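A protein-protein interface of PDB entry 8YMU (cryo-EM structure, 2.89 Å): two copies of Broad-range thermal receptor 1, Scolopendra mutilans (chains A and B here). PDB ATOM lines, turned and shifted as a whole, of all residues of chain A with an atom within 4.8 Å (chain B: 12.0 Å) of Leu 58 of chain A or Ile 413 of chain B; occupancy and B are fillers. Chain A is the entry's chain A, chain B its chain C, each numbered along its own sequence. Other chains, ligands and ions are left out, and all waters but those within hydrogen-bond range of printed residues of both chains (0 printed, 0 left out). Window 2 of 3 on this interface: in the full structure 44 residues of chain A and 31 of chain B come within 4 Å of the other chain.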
ATOM      1  N   ARG A  53      12.626  -4.491 -27.118  1.00  0.00           N
ATOM      2  CA  ARG A  53      13.056  -3.852 -28.353  1.00  0.00           C
ATOM      3  C   ARG A  53      11.981  -2.915 -28.889  1.00  0.00           C
ATOM      4  O   ARG A  53      12.251  -1.754 -29.191  1.00  0.00           O
ATOM      5  CB  ARG A  53      13.413  -4.906 -29.405  1.00  0.00           C
ATOM      6  CG  ARG A  53      12.280  -5.867 -29.732  1.00  0.00           C
ATOM      7  CD  ARG A  53      12.600  -6.717 -30.949  1.00  0.00           C
ATOM      8  NE  ARG A  53      11.504  -7.619 -31.282  1.00  0.00           N
ATOM      9  CZ  ARG A  53      10.445  -7.275 -32.002  1.00  0.00           C
ATOM     10  NH1 ARG A  53      10.305  -6.053 -32.485  1.00  0.00           N
ATOM     11  NH2 ARG A  53       9.502  -8.183 -32.242  1.00  0.00           N
ATOM     12  N   TRP A  54      10.756  -3.426 -29.003  1.00  0.00           N
ATOM     13  CA  TRP A  54       9.660  -2.658 -29.582  1.00  0.00           C
ATOM     14  C   TRP A  54       9.330  -1.416 -28.762  1.00  0.00           C
ATOM     15  O   TRP A  54       9.482  -0.289 -29.246  1.00  0.00           O
ATOM     16  CB  TRP A  54       8.414  -3.536 -29.720  1.00  0.00           C
ATOM     17  CG  TRP A  54       7.227  -2.802 -30.261  1.00  0.00           C
ATOM     18  CD1 TRP A  54       6.184  -2.290 -29.545  1.00  0.00           C
ATOM     19  CD2 TRP A  54       6.961  -2.495 -31.634  1.00  0.00           C
ATOM     20  NE1 TRP A  54       5.284  -1.685 -30.388  1.00  0.00           N
ATOM     21  CE2 TRP A  54       5.737  -1.796 -31.676  1.00  0.00           C
ATOM     22  CE3 TRP A  54       7.636  -2.744 -32.832  1.00  0.00           C
ATOM     23  CZ2 TRP A  54       5.176  -1.345 -32.869  1.00  0.00           C
ATOM     24  CZ3 TRP A  54       7.079  -2.294 -34.016  1.00  0.00           C
ATOM     25  CH2 TRP A  54       5.861  -1.602 -34.024  1.00  0.00           C
ATOM     26  N   GLN A  55       8.884  -1.607 -27.517  1.00  0.00           N
ATOM     27  CA  GLN A  55       8.352  -0.484 -26.752  1.00  0.00           C
ATOM     28  C   GLN A  55       9.469   0.430 -26.263  1.00  0.00           C
ATOM     29  O   GLN A  55       9.319   1.656 -26.243  1.00  0.00           O
ATOM     30  CB  GLN A  55       7.503  -0.994 -25.583  1.00  0.00           C
ATOM     31  CG  GLN A  55       8.273  -1.560 -24.404  1.00  0.00           C
ATOM     32  CD  GLN A  55       8.316  -0.590 -23.237  1.00  0.00           C
ATOM     33  OE1 GLN A  55       7.491   0.319 -23.145  1.00  0.00           O
ATOM     34  NE2 GLN A  55       9.261  -0.791 -22.329  1.00  0.00           N
ATOM     35  N   ARG A  56      10.605  -0.150 -25.864  1.00  0.00           N
ATOM     36  CA  ARG A  56      11.743   0.678 -25.473  1.00  0.00           C
ATOM     37  C   ARG A  56      12.225   1.538 -26.636  1.00  0.00           C
ATOM     38  O   ARG A  56      12.476   2.739 -26.470  1.00  0.00           O
ATOM     39  CB  ARG A  56      12.881  -0.192 -24.936  1.00  0.00           C
ATOM     40  CG  ARG A  56      12.717  -0.601 -23.478  1.00  0.00           C
ATOM     41  CD  ARG A  56      11.810  -1.808 -23.289  1.00  0.00           C
ATOM     42  NE  ARG A  56      12.363  -3.032 -23.853  1.00  0.00           N
ATOM     43  CZ  ARG A  56      11.675  -4.151 -24.026  1.00  0.00           C
ATOM     44  NH1 ARG A  56      10.386  -4.223 -23.734  1.00  0.00           N
ATOM     45  NH2 ARG A  56      12.295  -5.231 -24.495  1.00  0.00           N
ATOM     46  N   ALA A  57      12.354   0.944 -27.825  1.00  0.00           N
ATOM     47  CA  ALA A  57      12.778   1.715 -28.990  1.00  0.00           C
ATOM     48  C   ALA A  57      11.751   2.779 -29.351  1.00  0.00           C
ATOM     49  O   ALA A  57      12.116   3.898 -29.731  1.00  0.00           O
ATOM     50  CB  ALA A  57      13.031   0.785 -30.176  1.00  0.00           C
ATOM     51  N   LEU A  58      10.461   2.450 -29.250  1.00  0.00           N
ATOM     52  CA  LEU A  58       9.430   3.438 -29.552  1.00  0.00           C
ATOM     53  C   LEU A  58       9.486   4.604 -28.575  1.00  0.00           C
ATOM     54  O   LEU A  58       9.346   5.765 -28.976  1.00  0.00           O
ATOM     55  CB  LEU A  58       8.049   2.781 -29.532  1.00  0.00           C
ATOM     56  CG  LEU A  58       6.907   3.607 -30.130  1.00  0.00           C
ATOM     57  CD1 LEU A  58       5.832   2.695 -30.701  1.00  0.00           C
ATOM     58  CD2 LEU A  58       6.319   4.555 -29.096  1.00  0.00           C
ATOM     59  N   TRP A  59       9.686   4.317 -27.287  1.00  0.00           N
ATOM     60  CA  TRP A  59       9.820   5.376 -26.293  1.00  0.00           C
ATOM     61  C   TRP A  59      11.036   6.244 -26.586  1.00  0.00           C
ATOM     62  O   TRP A  59      10.976   7.477 -26.512  1.00  0.00           O
ATOM     63  CB  TRP A  59       9.916   4.766 -24.892  1.00  0.00           C
ATOM     64  CG  TRP A  59       9.993   5.784 -23.794  1.00  0.00           C
ATOM     65  CD1 TRP A  59       8.969   6.542 -23.305  1.00  0.00           C
ATOM     66  CD2 TRP A  59      11.160   6.159 -23.051  1.00  0.00           C
ATOM     67  NE1 TRP A  59       9.425   7.363 -22.301  1.00  0.00           N
ATOM     68  CE2 TRP A  59      10.767   7.146 -22.127  1.00  0.00           C
ATOM     69  CE3 TRP A  59      12.498   5.754 -23.078  1.00  0.00           C
ATOM     70  CZ2 TRP A  59      11.663   7.736 -21.237  1.00  0.00           C
ATOM     71  CZ3 TRP A  59      13.386   6.339 -22.193  1.00  0.00           C
ATOM     72  CH2 TRP A  59      12.965   7.320 -21.285  1.00  0.00           C
ATOM     73  N   PHE A  60      12.160   5.608 -26.922  1.00  0.00           N
ATOM     74  CA  PHE A  60      13.363   6.354 -27.273  1.00  0.00           C
ATOM     75  C   PHE A  60      13.094   7.291 -28.445  1.00  0.00           C
ATOM     76  O   PHE A  60      13.444   8.477 -28.407  1.00  0.00           O
ATOM     77  CB  PHE A  60      14.498   5.377 -27.600  1.00  0.00           C
ATOM     78  CG  PHE A  60      15.831   6.039 -27.824  1.00  0.00           C
ATOM     79  CD1 PHE A  60      16.106   6.698 -29.013  1.00  0.00           C
ATOM     80  CD2 PHE A  60      16.812   5.997 -26.848  1.00  0.00           C
ATOM     81  CE1 PHE A  60      17.330   7.302 -29.221  1.00  0.00           C
ATOM     82  CE2 PHE A  60      18.039   6.601 -27.051  1.00  0.00           C
ATOM     83  CZ  PHE A  60      18.298   7.254 -28.239  1.00  0.00           C
ATOM     84  N   ALA A  61      12.466   6.766 -29.499  1.00  0.00           N
ATOM     85  CA  ALA A  61      12.197   7.574 -30.683  1.00  0.00           C
ATOM     86  C   ALA A  61      11.256   8.729 -30.359  1.00  0.00           C
ATOM     87  O   ALA A  61      11.508   9.876 -30.746  1.00  0.00           O
ATOM     88  CB  ALA A  61      11.611   6.698 -31.790  1.00  0.00           C
ATOM     89  N   GLY A  62      10.175   8.448 -29.633  1.00  0.00           N
ATOM     90  CA  GLY A  62       9.180   9.450 -29.316  1.00  0.00           C
ATOM     91  C   GLY A  62       9.599  10.465 -28.283  1.00  0.00           C
ATOM     92  O   GLY A  62       8.965  11.518 -28.169  1.00  0.00           O
ATOM     93  N   ILE B 402       2.254  17.550 -25.958  1.00  0.00           N
ATOM     94  CA  ILE B 402       2.958  16.790 -26.991  1.00  0.00           C
ATOM     95  C   ILE B 402       3.647  15.556 -26.420  1.00  0.00           C
ATOM     96  O   ILE B 402       3.291  14.423 -26.763  1.00  0.00           O
ATOM     97  CB  ILE B 402       3.973  17.685 -27.723  1.00  0.00           C
ATOM     98  CG1 ILE B 402       3.263  18.883 -28.355  1.00  0.00           C
ATOM     99  CG2 ILE B 402       4.718  16.885 -28.781  1.00  0.00           C
ATOM    100  CD1 ILE B 402       2.207  18.503 -29.367  1.00  0.00           C
ATOM    101  N   LEU B 403       4.641  15.765 -25.554  1.00  0.00           N
ATOM    102  CA  LEU B 403       5.331  14.635 -24.939  1.00  0.00           C
ATOM    103  C   LEU B 403       4.342  13.712 -24.241  1.00  0.00           C
ATOM    104  O   LEU B 403       4.426  12.484 -24.368  1.00  0.00           O
ATOM    105  CB  LEU B 403       6.391  15.140 -23.958  1.00  0.00           C
ATOM    106  CG  LEU B 403       7.287  14.085 -23.304  1.00  0.00           C
ATOM    107  CD1 LEU B 403       8.658  14.667 -22.995  1.00  0.00           C
ATOM    108  CD2 LEU B 403       6.641  13.540 -22.041  1.00  0.00           C
ATOM    109  N   SER B 404       3.393  14.286 -23.501  1.00  0.00           N
ATOM    110  CA  SER B 404       2.319  13.478 -22.936  1.00  0.00           C
ATOM    111  C   SER B 404       1.491  12.833 -24.040  1.00  0.00           C
ATOM    112  O   SER B 404       1.014  11.704 -23.889  1.00  0.00           O
ATOM    113  CB  SER B 404       1.437  14.333 -22.026  1.00  0.00           C
ATOM    114  OG  SER B 404       2.159  14.776 -20.890  1.00  0.00           O
ATOM    115  N   VAL B 405       1.319  13.532 -25.164  1.00  0.00           N
ATOM    116  CA  VAL B 405       0.604  12.950 -26.296  1.00  0.00           C
ATOM    117  C   VAL B 405       1.362  11.749 -26.845  1.00  0.00           C
ATOM    118  O   VAL B 405       0.765  10.714 -27.168  1.00  0.00           O
ATOM    119  CB  VAL B 405       0.365  14.014 -27.383  1.00  0.00           C
ATOM    120  CG1 VAL B 405      -0.302  13.389 -28.596  1.00  0.00           C
ATOM    121  CG2 VAL B 405      -0.478  15.153 -26.832  1.00  0.00           C
ATOM    122  N   ILE B 406       2.685  11.866 -26.970  1.00  0.00           N
ATOM    123  CA  ILE B 406       3.486  10.742 -27.446  1.00  0.00           C
ATOM    124  C   ILE B 406       3.402   9.575 -26.473  1.00  0.00           C
ATOM    125  O   ILE B 406       3.296   8.412 -26.883  1.00  0.00           O
ATOM    126  CB  ILE B 406       4.943  11.183 -27.677  1.00  0.00           C
ATOM    127  CG1 ILE B 406       5.006  12.291 -28.730  1.00  0.00           C
ATOM    128  CG2 ILE B 406       5.798   9.998 -28.096  1.00  0.00           C
ATOM    129  CD1 ILE B 406       4.495  11.869 -30.090  1.00  0.00           C
ATOM    130  N   GLU B 407       3.455   9.859 -25.170  1.00  0.00           N
ATOM    131  CA  GLU B 407       3.350   8.795 -24.177  1.00  0.00           C
ATOM    132  C   GLU B 407       1.994   8.103 -24.262  1.00  0.00           C
ATOM    133  O   GLU B 407       1.902   6.873 -24.168  1.00  0.00           O
ATOM    134  CB  GLU B 407       3.584   9.361 -22.776  1.00  0.00           C
ATOM    135  CG  GLU B 407       3.749   8.304 -21.699  1.00  0.00           C
ATOM    136  CD  GLU B 407       5.029   7.507 -21.859  1.00  0.00           C
ATOM    137  OE1 GLU B 407       5.990   8.038 -22.452  1.00  0.00           O
ATOM    138  OE2 GLU B 407       5.073   6.350 -21.392  1.00  0.00           O
ATOM    139  N   VAL B 408       0.925   8.882 -24.440  1.00  0.00           N
ATOM    140  CA  VAL B 408      -0.411   8.306 -24.566  1.00  0.00           C
ATOM    141  C   VAL B 408      -0.515   7.452 -25.820  1.00  0.00           C
ATOM    142  O   VAL B 408      -1.121   6.374 -25.798  1.00  0.00           O
ATOM    143  CB  VAL B 408      -1.476   9.420 -24.552  1.00  0.00           C
ATOM    144  CG1 VAL B 408      -2.854   8.838 -24.823  1.00  0.00           C
ATOM    145  CG2 VAL B 408      -1.453  10.159 -23.223  1.00  0.00           C
ATOM    146  N   PHE B 409       0.056   7.918 -26.933  1.00  0.00           N
ATOM    147  CA  PHE B 409       0.041   7.123 -28.155  1.00  0.00           C
ATOM    148  C   PHE B 409       0.803   5.816 -27.972  1.00  0.00           C
ATOM    149  O   PHE B 409       0.358   4.759 -28.436  1.00  0.00           O
ATOM    150  CB  PHE B 409       0.627   7.929 -29.314  1.00  0.00           C
ATOM    151  CG  PHE B 409      -0.397   8.711 -30.086  1.00  0.00           C
ATOM    152  CD1 PHE B 409      -1.001   9.826 -29.529  1.00  0.00           C
ATOM    153  CD2 PHE B 409      -0.756   8.330 -31.368  1.00  0.00           C
ATOM    154  CE1 PHE B 409      -1.943  10.546 -30.237  1.00  0.00           C
ATOM    155  CE2 PHE B 409      -1.698   9.048 -32.082  1.00  0.00           C
ATOM    156  CZ  PHE B 409      -2.292  10.157 -31.515  1.00  0.00           C
ATOM    157  N   GLU B 410       1.956   5.868 -27.300  1.00  0.00           N
ATOM    158  CA  GLU B 410       2.708   4.647 -27.034  1.00  0.00           C
ATOM    159  C   GLU B 410       1.909   3.693 -26.154  1.00  0.00           C
ATOM    160  O   GLU B 410       1.902   2.478 -26.388  1.00  0.00           O
ATOM    161  CB  GLU B 410       4.049   4.987 -26.383  1.00  0.00           C
ATOM    162  CG  GLU B 410       4.996   3.803 -26.242  1.00  0.00           C
ATOM    163  CD  GLU B 410       4.739   2.991 -24.987  1.00  0.00           C
ATOM    164  OE1 GLU B 410       4.251   3.569 -23.993  1.00  0.00           O
ATOM    165  OE2 GLU B 410       5.023   1.775 -24.995  1.00  0.00           O
ATOM    166  N   VAL B 411       1.232   4.225 -25.136  1.00  0.00           N
ATOM    167  CA  VAL B 411       0.408   3.387 -24.269  1.00  0.00           C
ATOM    168  C   VAL B 411      -0.706   2.730 -25.075  1.00  0.00           C
ATOM    169  O   VAL B 411      -1.003   1.541 -24.910  1.00  0.00           O
ATOM    170  CB  VAL B 411      -0.153   4.212 -23.097  1.00  0.00           C
ATOM    171  CG1 VAL B 411      -1.201   3.413 -22.339  1.00  0.00           C
ATOM    172  CG2 VAL B 411       0.971   4.646 -22.169  1.00  0.00           C
ATOM    173  N   VAL B 412      -1.342   3.500 -25.960  1.00  0.00           N
ATOM    174  CA  VAL B 412      -2.405   2.950 -26.795  1.00  0.00           C
ATOM    175  C   VAL B 412      -1.865   1.845 -27.692  1.00  0.00           C
ATOM    176  O   VAL B 412      -2.500   0.793 -27.844  1.00  0.00           O
ATOM    177  CB  VAL B 412      -3.073   4.066 -27.618  1.00  0.00           C
ATOM    178  CG1 VAL B 412      -3.867   3.472 -28.771  1.00  0.00           C
ATOM    179  CG2 VAL B 412      -3.967   4.916 -26.728  1.00  0.00           C
ATOM    180  N   ILE B 413      -0.693   2.055 -28.301  1.00  0.00           N
ATOM    181  CA  ILE B 413      -0.062   1.007 -29.100  1.00  0.00           C
ATOM    182  C   ILE B 413       0.562  -0.080 -28.239  1.00  0.00           C
ATOM    183  O   ILE B 413       0.862  -1.168 -28.754  1.00  0.00           O
ATOM    184  CB  ILE B 413       1.014   1.591 -30.037  1.00  0.00           C
ATOM    185  CG1 ILE B 413       1.366   0.582 -31.133  1.00  0.00           C
ATOM    186  CG2 ILE B 413       2.256   1.975 -29.250  1.00  0.00           C
ATOM    187  CD1 ILE B 413       0.231   0.303 -32.091  1.00  0.00           C
ATOM    188  N   PHE B 414       0.763   0.173 -26.950  1.00  0.00           N
ATOM    189  CA  PHE B 414       1.304  -0.828 -26.038  1.00  0.00           C
ATOM    190  C   PHE B 414       2.674  -1.314 -26.497  1.00  0.00           C
ATOM    191  O   PHE B 414       3.704  -0.867 -25.989  1.00  0.00           O
ATOM    192  CB  PHE B 414       0.338  -2.010 -25.913  1.00  0.00           C
ATOM    193  CG  PHE B 414      -0.835  -1.739 -25.014  1.00  0.00           C
ATOM    194  CD1 PHE B 414      -0.650  -1.199 -23.753  1.00  0.00           C
ATOM    195  CD2 PHE B 414      -2.125  -2.021 -25.433  1.00  0.00           C
ATOM    196  CE1 PHE B 414      -1.728  -0.949 -22.925  1.00  0.00           C
ATOM    197  CE2 PHE B 414      -3.206  -1.772 -24.611  1.00  0.00           C
ATOM    198  CZ  PHE B 414      -3.007  -1.236 -23.355  1.00  0.00           C
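No position is printed for both chains. Of the 6 pairs that touch across the chains among the printed residues, none has its exchanged pair printed and touching as well.
Of the 13 printed residues of chain B, 5 touch a printed residue of chain A. Of the 10 printed residues of chain A, 4 touch a printed residue of chain B. Hydrophobic or aromatic side chains of chain A within 4 Å of the printed part of chain B: Leu 58 and Trp 59. Among the printed residues, 6 pairs touch across the chains. Among the printed residues, no Asp or Glu carboxylate lies within 4 Å of a Lys or Arg side-chain nitrogen of the other chain.
The side-chain amide oxygen (OE1) of Gln 55 of chain A sits close to the side-chain carboxylate (OE2) of Glu 410 of chain B.
Of chain B, only Glu 410 (3.2 Å) and Ile 413 (3.9 Å) come within 4 Å of Leu 58 of chain A. Ile 413 of chain B touches just one residue of chain A: Leu 58. Of chain B, only Glu 410 (3.4 Å) and Phe 414 (3.8 Å) come within 4 Å of Gln 55 of chain A. Ala 57 of chain A touches none of the printed residues of chain B. No residue of chain B comes within 4 Å of Ala 61 of chain A. Of chain B, only Ile 406 (3.5 Å) comes within 4 Å of Gly 62 of chain A. Printed residues of chain A within 4 Å of Phe 414 of chain B: Gln 55. Of the printed residues of chain A, Glu 407 of chain B touches Trp 59 (3.4 Å). Of the printed residues of chain A, Ile 406 of chain B touches Gly 62. Of the printed residues of chain A, Glu 410 of chain B touches Gln 55 (3.4 Å) and Leu 58 (3.2 Å). Val 408 of chain B touches none of the printed residues of chain A. Val 405 of chain B touches none of the printed residues of chain A. The nearest residue of chain B that does not touch Leu 58 of chain A is Ile 406 of chain B (5.4 Å).
Among the printed residues, merely in contact across the chains: Gln 55 of chain A with Phe 414 of chain B (3.8 Å), Leu 58 of chain A with Glu 410 of chain B (3.2 Å), Leu 58 of chain A with Ile 413 of chain B (3.9 Å), Trp 59 of chain A with Glu 407 of chain B (3.4 Å) and Gly 62 of chain A with Ile 406 of chain B (3.5 Å).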
